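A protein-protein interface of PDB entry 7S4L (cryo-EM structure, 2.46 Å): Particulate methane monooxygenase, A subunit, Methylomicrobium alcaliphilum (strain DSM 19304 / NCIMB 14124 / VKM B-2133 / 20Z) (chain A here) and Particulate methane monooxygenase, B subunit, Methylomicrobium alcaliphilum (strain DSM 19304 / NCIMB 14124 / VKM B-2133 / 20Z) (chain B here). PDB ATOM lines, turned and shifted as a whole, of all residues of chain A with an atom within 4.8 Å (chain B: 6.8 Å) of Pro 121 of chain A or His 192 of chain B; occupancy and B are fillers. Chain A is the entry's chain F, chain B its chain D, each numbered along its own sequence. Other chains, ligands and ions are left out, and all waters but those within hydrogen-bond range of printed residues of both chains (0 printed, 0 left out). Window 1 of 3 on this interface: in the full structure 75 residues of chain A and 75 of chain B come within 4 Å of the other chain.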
ATOM      1  N   ASP A  49      26.551 -11.516 -19.637  1.00  0.00           N
ATOM      2  CA  ASP A  49      26.146 -10.153 -19.202  1.00  0.00           C
ATOM      3  C   ASP A  49      24.619 -10.044 -19.134  1.00  0.00           C
ATOM      4  O   ASP A  49      24.139  -9.237 -18.315  1.00  0.00           O
ATOM      5  CB  ASP A  49      26.731  -9.084 -20.128  1.00  0.00           C
ATOM      6  CG  ASP A  49      26.859  -7.705 -19.506  1.00  0.00           C
ATOM      7  OD1 ASP A  49      27.984  -7.318 -19.174  1.00  0.00           O
ATOM      8  OD2 ASP A  49      25.841  -7.020 -19.378  1.00  0.00           O
ATOM      9  N   LYS A  55      26.311 -15.705 -14.780  1.00  0.00           N
ATOM     10  CA  LYS A  55      27.496 -15.093 -14.196  1.00  0.00           C
ATOM     11  C   LYS A  55      28.132 -16.092 -13.238  1.00  0.00           C
ATOM     12  O   LYS A  55      28.016 -16.002 -12.017  1.00  0.00           O
ATOM     13  CB  LYS A  55      27.129 -13.788 -13.507  1.00  0.00           C
ATOM     14  CG  LYS A  55      26.636 -12.729 -14.464  1.00  0.00           C
ATOM     15  CD  LYS A  55      26.014 -11.572 -13.732  1.00  0.00           C
ATOM     16  CE  LYS A  55      25.926 -10.350 -14.614  1.00  0.00           C
ATOM     17  NZ  LYS A  55      25.251 -10.641 -15.894  1.00  0.00           N
ATOM     18  N   LEU A  97      28.455   1.079 -20.374  1.00  0.00           N
ATOM     19  CA  LEU A  97      27.510   0.888 -19.284  1.00  0.00           C
ATOM     20  C   LEU A  97      26.235   1.678 -19.512  1.00  0.00           C
ATOM     21  O   LEU A  97      25.143   1.190 -19.220  1.00  0.00           O
ATOM     22  CB  LEU A  97      28.152   1.279 -17.958  1.00  0.00           C
ATOM     23  CG  LEU A  97      28.642   0.092 -17.139  1.00  0.00           C
ATOM     24  CD1 LEU A  97      27.470  -0.698 -16.630  1.00  0.00           C
ATOM     25  CD2 LEU A  97      29.533  -0.786 -17.977  1.00  0.00           C
ATOM     26  N   GLU A 100      24.193  -0.224 -22.142  1.00  0.00           N
ATOM     27  CA  GLU A 100      23.653  -1.460 -21.602  1.00  0.00           C
ATOM     28  C   GLU A 100      22.525  -1.191 -20.623  1.00  0.00           C
ATOM     29  O   GLU A 100      21.516  -1.898 -20.629  1.00  0.00           O
ATOM     30  CB  GLU A 100      24.759  -2.264 -20.937  1.00  0.00           C
ATOM     31  CG  GLU A 100      25.657  -2.946 -21.927  1.00  0.00           C
ATOM     32  CD  GLU A 100      26.623  -3.893 -21.272  1.00  0.00           C
ATOM     33  OE1 GLU A 100      27.036  -3.622 -20.128  1.00  0.00           O
ATOM     34  OE2 GLU A 100      26.972  -4.912 -21.899  1.00  0.00           O
ATOM     35  N   TRP A 101      22.668  -0.179 -19.771  1.00  0.00           N
ATOM     36  CA  TRP A 101      21.620   0.080 -18.795  1.00  0.00           C
ATOM     37  C   TRP A 101      20.366   0.607 -19.462  1.00  0.00           C
ATOM     38  O   TRP A 101      19.253   0.217 -19.098  1.00  0.00           O
ATOM     39  CB  TRP A 101      22.114   1.052 -17.732  1.00  0.00           C
ATOM     40  CG  TRP A 101      22.542   0.348 -16.509  1.00  0.00           C
ATOM     41  CD1 TRP A 101      23.805   0.236 -16.036  1.00  0.00           C
ATOM     42  CD2 TRP A 101      21.707  -0.374 -15.607  1.00  0.00           C
ATOM     43  NE1 TRP A 101      23.813  -0.504 -14.886  1.00  0.00           N
ATOM     44  CE2 TRP A 101      22.534  -0.891 -14.601  1.00  0.00           C
ATOM     45  CE3 TRP A 101      20.339  -0.629 -15.549  1.00  0.00           C
ATOM     46  CZ2 TRP A 101      22.042  -1.646 -13.552  1.00  0.00           C
ATOM     47  CZ3 TRP A 101      19.855  -1.378 -14.510  1.00  0.00           C
ATOM     48  CH2 TRP A 101      20.700  -1.877 -13.525  1.00  0.00           C
ATOM     49  N   ARG A 104      18.734  -2.483 -20.954  1.00  0.00           N
ATOM     50  CA  ARG A 104      18.166  -3.383 -19.959  1.00  0.00           C
ATOM     51  C   ARG A 104      16.902  -2.803 -19.355  1.00  0.00           C
ATOM     52  O   ARG A 104      15.914  -3.515 -19.163  1.00  0.00           O
ATOM     53  CB  ARG A 104      19.172  -3.675 -18.851  1.00  0.00           C
ATOM     54  CG  ARG A 104      20.517  -4.140 -19.316  1.00  0.00           C
ATOM     55  CD  ARG A 104      20.428  -5.396 -20.121  1.00  0.00           C
ATOM     56  NE  ARG A 104      21.678  -5.644 -20.821  1.00  0.00           N
ATOM     57  CZ  ARG A 104      22.695  -6.314 -20.303  1.00  0.00           C
ATOM     58  NH1 ARG A 104      22.607  -6.806 -19.082  1.00  0.00           N
ATOM     59  NH2 ARG A 104      23.798  -6.492 -21.005  1.00  0.00           N
ATOM     60  N   VAL A 119      18.635  -9.090 -15.005  1.00  0.00           N
ATOM     61  CA  VAL A 119      19.300  -8.792 -16.265  1.00  0.00           C
ATOM     62  C   VAL A 119      20.274  -7.629 -16.148  1.00  0.00           C
ATOM     63  O   VAL A 119      20.713  -7.085 -17.164  1.00  0.00           O
ATOM     64  CB  VAL A 119      18.265  -8.496 -17.361  1.00  0.00           C
ATOM     65  CG1 VAL A 119      17.400  -9.700 -17.598  1.00  0.00           C
ATOM     66  CG2 VAL A 119      17.423  -7.314 -16.964  1.00  0.00           C
ATOM     67  N   PHE A 120      20.629  -7.234 -14.933  1.00  0.00           N
ATOM     68  CA  PHE A 120      21.520  -6.098 -14.794  1.00  0.00           C
ATOM     69  C   PHE A 120      22.882  -6.416 -15.404  1.00  0.00           C
ATOM     70  O   PHE A 120      23.265  -7.581 -15.518  1.00  0.00           O
ATOM     71  CB  PHE A 120      21.678  -5.709 -13.332  1.00  0.00           C
ATOM     72  CG  PHE A 120      22.171  -6.812 -12.462  1.00  0.00           C
ATOM     73  CD1 PHE A 120      23.512  -7.102 -12.386  1.00  0.00           C
ATOM     74  CD2 PHE A 120      21.294  -7.551 -11.707  1.00  0.00           C
ATOM     75  CE1 PHE A 120      23.965  -8.109 -11.584  1.00  0.00           C
ATOM     76  CE2 PHE A 120      21.745  -8.560 -10.904  1.00  0.00           C
ATOM     77  CZ  PHE A 120      23.080  -8.839 -10.843  1.00  0.00           C
ATOM     78  N   PRO A 121      23.629  -5.398 -15.809  1.00  0.00           N
ATOM     79  CA  PRO A 121      24.876  -5.628 -16.539  1.00  0.00           C
ATOM     80  C   PRO A 121      26.044  -5.917 -15.607  1.00  0.00           C
ATOM     81  O   PRO A 121      25.961  -5.779 -14.391  1.00  0.00           O
ATOM     82  CB  PRO A 121      25.098  -4.309 -17.286  1.00  0.00           C
ATOM     83  CG  PRO A 121      23.902  -3.469 -17.001  1.00  0.00           C
ATOM     84  CD  PRO A 121      23.299  -3.973 -15.755  1.00  0.00           C
ATOM     85  N   SER A 122      27.154  -6.315 -16.218  1.00  0.00           N
ATOM     86  CA  SER A 122      28.388  -6.503 -15.477  1.00  0.00           C
ATOM     87  C   SER A 122      28.991  -5.154 -15.108  1.00  0.00           C
ATOM     88  O   SER A 122      28.680  -4.121 -15.701  1.00  0.00           O
ATOM     89  CB  SER A 122      29.393  -7.303 -16.296  1.00  0.00           C
ATOM     90  OG  SER A 122      28.813  -8.496 -16.778  1.00  0.00           O
ATOM     91  N   ASN A 123      29.864  -5.135 -14.100  1.00  0.00           N
ATOM     92  CA  ASN A 123      30.497  -3.862 -13.652  1.00  0.00           C
ATOM     93  C   ASN A 123      31.953  -3.852 -14.125  1.00  0.00           C
ATOM     94  O   ASN A 123      32.713  -4.746 -13.702  1.00  0.00           O
ATOM     95  CB  ASN A 123      30.337  -3.641 -12.146  1.00  0.00           C
ATOM     96  CG  ASN A 123      31.098  -2.443 -11.619  1.00  0.00           C
ATOM     97  OD1 ASN A 123      31.043  -1.358 -12.194  1.00  0.00           O
ATOM     98  ND2 ASN A 123      31.802  -2.631 -10.514  1.00  0.00           N
ATOM     99  N   ILE A 163      27.722  -7.355  -5.781  1.00  0.00           N
ATOM    100  CA  ILE A 163      26.449  -7.129  -6.449  1.00  0.00           C
ATOM    101  C   ILE A 163      25.676  -8.423  -6.630  1.00  0.00           C
ATOM    102  O   ILE A 163      24.456  -8.448  -6.474  1.00  0.00           O
ATOM    103  CB  ILE A 163      26.687  -6.429  -7.796  1.00  0.00           C
ATOM    104  CG1 ILE A 163      27.708  -5.310  -7.635  1.00  0.00           C
ATOM    105  CG2 ILE A 163      25.398  -5.873  -8.331  1.00  0.00           C
ATOM    106  CD1 ILE A 163      28.032  -4.611  -8.916  1.00  0.00           C
ATOM    107  N   GLY B 187      20.612  -3.161  -3.654  1.00  0.00           N
ATOM    108  CA  GLY B 187      22.048  -3.363  -3.701  1.00  0.00           C
ATOM    109  C   GLY B 187      22.608  -3.173  -5.095  1.00  0.00           C
ATOM    110  O   GLY B 187      23.620  -2.493  -5.281  1.00  0.00           O
ATOM    111  N   VAL B 188      21.958  -3.772  -6.092  1.00  0.00           N
ATOM    112  CA  VAL B 188      22.389  -3.594  -7.473  1.00  0.00           C
ATOM    113  C   VAL B 188      22.402  -2.120  -7.835  1.00  0.00           C
ATOM    114  O   VAL B 188      23.396  -1.594  -8.354  1.00  0.00           O
ATOM    115  CB  VAL B 188      21.477  -4.392  -8.419  1.00  0.00           C
ATOM    116  CG1 VAL B 188      21.844  -4.111  -9.854  1.00  0.00           C
ATOM    117  CG2 VAL B 188      21.575  -5.864  -8.125  1.00  0.00           C
ATOM    118  N   TYR B 189      21.293  -1.433  -7.575  1.00  0.00           N
ATOM    119  CA  TYR B 189      21.210  -0.021  -7.924  1.00  0.00           C
ATOM    120  C   TYR B 189      22.309   0.772  -7.238  1.00  0.00           C
ATOM    121  O   TYR B 189      23.018   1.553  -7.876  1.00  0.00           O
ATOM    122  CB  TYR B 189      19.841   0.533  -7.555  1.00  0.00           C
ATOM    123  CG  TYR B 189      18.777   0.230  -8.568  1.00  0.00           C
ATOM    124  CD1 TYR B 189      19.106  -0.042  -9.879  1.00  0.00           C
ATOM    125  CD2 TYR B 189      17.443   0.211  -8.213  1.00  0.00           C
ATOM    126  CE1 TYR B 189      18.139  -0.321 -10.808  1.00  0.00           C
ATOM    127  CE2 TYR B 189      16.471  -0.067  -9.134  1.00  0.00           C
ATOM    128  CZ  TYR B 189      16.822  -0.332 -10.428  1.00  0.00           C
ATOM    129  OH  TYR B 189      15.846  -0.609 -11.349  1.00  0.00           O
ATOM    130  N   GLY B 190      22.464   0.587  -5.928  1.00  0.00           N
ATOM    131  CA  GLY B 190      23.454   1.353  -5.200  1.00  0.00           C
ATOM    132  C   GLY B 190      24.854   1.136  -5.726  1.00  0.00           C
ATOM    133  O   GLY B 190      25.588   2.088  -5.978  1.00  0.00           O
ATOM    134  N   TRP B 191      25.246  -0.124  -5.901  1.00  0.00           N
ATOM    135  CA  TRP B 191      26.612  -0.397  -6.328  1.00  0.00           C
ATOM    136  C   TRP B 191      26.872   0.143  -7.724  1.00  0.00           C
ATOM    137  O   TRP B 191      27.911   0.770  -7.973  1.00  0.00           O
ATOM    138  CB  TRP B 191      26.885  -1.895  -6.266  1.00  0.00           C
ATOM    139  CG  TRP B 191      27.291  -2.332  -4.914  1.00  0.00           C
ATOM    140  CD1 TRP B 191      26.658  -3.231  -4.124  1.00  0.00           C
ATOM    141  CD2 TRP B 191      28.421  -1.872  -4.178  1.00  0.00           C
ATOM    142  NE1 TRP B 191      27.325  -3.371  -2.936  1.00  0.00           N
ATOM    143  CE2 TRP B 191      28.416  -2.542  -2.947  1.00  0.00           C
ATOM    144  CE3 TRP B 191      29.440  -0.960  -4.442  1.00  0.00           C
ATOM    145  CZ2 TRP B 191      29.385  -2.330  -1.984  1.00  0.00           C
ATOM    146  CZ3 TRP B 191      30.399  -0.751  -3.489  1.00  0.00           C
ATOM    147  CH2 TRP B 191      30.367  -1.430  -2.275  1.00  0.00           C
ATOM    148  N   HIS B 192      25.948  -0.087  -8.655  1.00  0.00           N
ATOM    149  CA  HIS B 192      26.186   0.387 -10.009  1.00  0.00           C
ATOM    150  C   HIS B 192      26.200   1.906 -10.062  1.00  0.00           C
ATOM    151  O   HIS B 192      27.049   2.499 -10.734  1.00  0.00           O
ATOM    152  CB  HIS B 192      25.144  -0.187 -10.957  1.00  0.00           C
ATOM    153  CG  HIS B 192      25.514  -1.527 -11.500  1.00  0.00           C
ATOM    154  ND1 HIS B 192      26.280  -1.682 -12.631  1.00  0.00           N
ATOM    155  CD2 HIS B 192      25.249  -2.773 -11.052  1.00  0.00           C
ATOM    156  CE1 HIS B 192      26.460  -2.969 -12.866  1.00  0.00           C
ATOM    157  NE2 HIS B 192      25.844  -3.653 -11.921  1.00  0.00           N
ATOM    158  N   LEU B 193      25.287   2.556  -9.345  1.00  0.00           N
ATOM    159  CA  LEU B 193      25.286   4.011  -9.317  1.00  0.00           C
ATOM    160  C   LEU B 193      26.568   4.550  -8.709  1.00  0.00           C
ATOM    161  O   LEU B 193      27.115   5.546  -9.188  1.00  0.00           O
ATOM    162  CB  LEU B 193      24.079   4.516  -8.538  1.00  0.00           C
ATOM    163  CG  LEU B 193      24.034   6.025  -8.372  1.00  0.00           C
ATOM    164  CD1 LEU B 193      23.939   6.674  -9.727  1.00  0.00           C
ATOM    165  CD2 LEU B 193      22.862   6.417  -7.511  1.00  0.00           C
ATOM    166  N   PHE B 194      27.065   3.914  -7.651  1.00  0.00           N
ATOM    167  CA  PHE B 194      28.297   4.378  -7.035  1.00  0.00           C
ATOM    168  C   PHE B 194      29.461   4.284  -8.005  1.00  0.00           C
ATOM    169  O   PHE B 194      30.216   5.244  -8.182  1.00  0.00           O
ATOM    170  CB  PHE B 194      28.599   3.576  -5.774  1.00  0.00           C
ATOM    171  CG  PHE B 194      30.016   3.700  -5.322  1.00  0.00           C
ATOM    172  CD1 PHE B 194      30.410   4.760  -4.534  1.00  0.00           C
ATOM    173  CD2 PHE B 194      30.960   2.767  -5.696  1.00  0.00           C
ATOM    174  CE1 PHE B 194      31.711   4.881  -4.125  1.00  0.00           C
ATOM    175  CE2 PHE B 194      32.263   2.886  -5.288  1.00  0.00           C
ATOM    176  CZ  PHE B 194      32.638   3.945  -4.501  1.00  0.00           C
ATOM    177  N   TRP B 195      29.642   3.123  -8.626  1.00  0.00           N
ATOM    178  CA  TRP B 195      30.764   2.980  -9.546  1.00  0.00           C
ATOM    179  C   TRP B 195      30.637   3.941 -10.719  1.00  0.00           C
ATOM    180  O   TRP B 195      31.638   4.500 -11.186  1.00  0.00           O
ATOM    181  CB  TRP B 195      30.865   1.540 -10.030  1.00  0.00           C
ATOM    182  CG  TRP B 195      31.433   0.634  -9.005  1.00  0.00           C
ATOM    183  CD1 TRP B 195      30.797  -0.383  -8.376  1.00  0.00           C
ATOM    184  CD2 TRP B 195      32.757   0.669  -8.474  1.00  0.00           C
ATOM    185  NE1 TRP B 195      31.642  -0.994  -7.489  1.00  0.00           N
ATOM    186  CE2 TRP B 195      32.855  -0.363  -7.532  1.00  0.00           C
ATOM    187  CE3 TRP B 195      33.873   1.473  -8.710  1.00  0.00           C
ATOM    188  CZ2 TRP B 195      34.019  -0.614  -6.823  1.00  0.00           C
ATOM    189  CZ3 TRP B 195      35.024   1.221  -8.008  1.00  0.00           C
ATOM    190  CH2 TRP B 195      35.091   0.189  -7.076  1.00  0.00           C
ATOM    191  N   TYR B 196      29.414   4.167 -11.198  1.00  0.00           N
ATOM    192  CA  TYR B 196      29.232   5.093 -12.304  1.00  0.00           C
ATOM    193  C   TYR B 196      29.586   6.513 -11.896  1.00  0.00           C
ATOM    194  O   TYR B 196      30.261   7.229 -12.642  1.00  0.00           O
ATOM    195  CB  TYR B 196      27.798   5.031 -12.809  1.00  0.00           C
ATOM    196  CG  TYR B 196      27.674   5.454 -14.242  1.00  0.00           C
ATOM    197  CD1 TYR B 196      27.932   4.564 -15.263  1.00  0.00           C
ATOM    198  CD2 TYR B 196      27.312   6.745 -14.571  1.00  0.00           C
ATOM    199  CE1 TYR B 196      27.826   4.944 -16.572  1.00  0.00           C
ATOM    200  CE2 TYR B 196      27.204   7.133 -15.876  1.00  0.00           C
ATOM    201  CZ  TYR B 196      27.463   6.229 -16.873  1.00  0.00           C
ATOM    202  OH  TYR B 196      27.358   6.607 -18.186  1.00  0.00           O
ATOM    203  N   LEU B 197      29.125   6.948 -10.727  1.00  0.00           N
ATOM    204  CA  LEU B 197      29.469   8.286 -10.277  1.00  0.00           C
ATOM    205  C   LEU B 197      30.963   8.421 -10.049  1.00  0.00           C
ATOM    206  O   LEU B 197      31.524   9.494 -10.278  1.00  0.00           O
ATOM    207  CB  LEU B 197      28.703   8.627  -9.009  1.00  0.00           C
ATOM    208  CG  LEU B 197      27.219   8.852  -9.263  1.00  0.00           C
ATOM    209  CD1 LEU B 197      26.575   9.524  -8.074  1.00  0.00           C
ATOM    210  CD2 LEU B 197      27.037   9.678 -10.513  1.00  0.00           C
ATOM    211  N   LEU B 198      31.621   7.357  -9.605  1.00  0.00           N
ATOM    212  CA  LEU B 198      33.068   7.424  -9.450  1.00  0.00           C
ATOM    213  C   LEU B 198      33.751   7.641 -10.790  1.00  0.00           C
ATOM    214  O   LEU B 198      34.625   8.509 -10.917  1.00  0.00           O
ATOM    215  CB  LEU B 198      33.584   6.149  -8.794  1.00  0.00           C
ATOM    216  CG  LEU B 198      35.048   6.206  -8.381  1.00  0.00           C
ATOM    217  CD1 LEU B 198      35.234   7.278  -7.338  1.00  0.00           C
ATOM    218  CD2 LEU B 198      35.499   4.867  -7.855  1.00  0.00           C
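NE2 of His 192 of chain B sits close to O of Pro 121 of chain A, 3.3 Å away. The indole nitrogen (NE1) of Trp 195 of chain B sits close to the side-chain amide nitrogen (ND2) of Asn 123 of chain A (3.4 Å).
OD1 of Asp 49 of chain A lies within hydrogen-bond range of OG of Ser 122 of chain A (2.8 Å).
Printed residues of chain B within 4 Å of Leu 97 of chain A: Tyr 196. Of chain B, only His 192 (3.2 Å) comes within 4 Å of Pro 121 of chain A. Printed residues of chain B within 4 Å of Asn 123 of chain A: Trp 195 (3.3 Å).
Among the printed residues, pairs that only touch across the chains: Trp 101 of chain A with His 192 of chain B (3.5 Å), Phe 120 of chain A with Val 188 of chain B (3.8 Å), Ile 163 of chain A with Trp 191 of chain B (3.8 Å), Ser 122 of chain A with His 192 of chain B (3.8 Å), Ile 163 of chain A with Val 188 of chain B (3.8 Å), Ile 163 of chain A with His 192 of chain B (3.8 Å) and Leu 97 of chain A with Tyr 196 of chain B (3.9 Å).
Of the 12 printed residues of chain A, 7 touch a printed residue of chain B. Printed residues of chain A that touch a printed residue of chain B: Leu 97, Trp 101, Phe 120, Pro 121, Ser 122, Asn 123 and Ile 163. Hydrophobic or aromatic side chains of chain B that line the printed part of chain A: Val 188, Trp 191, His 192, Trp 195 and Tyr 196. Among the printed residues, 9 pairs touch across the chains.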
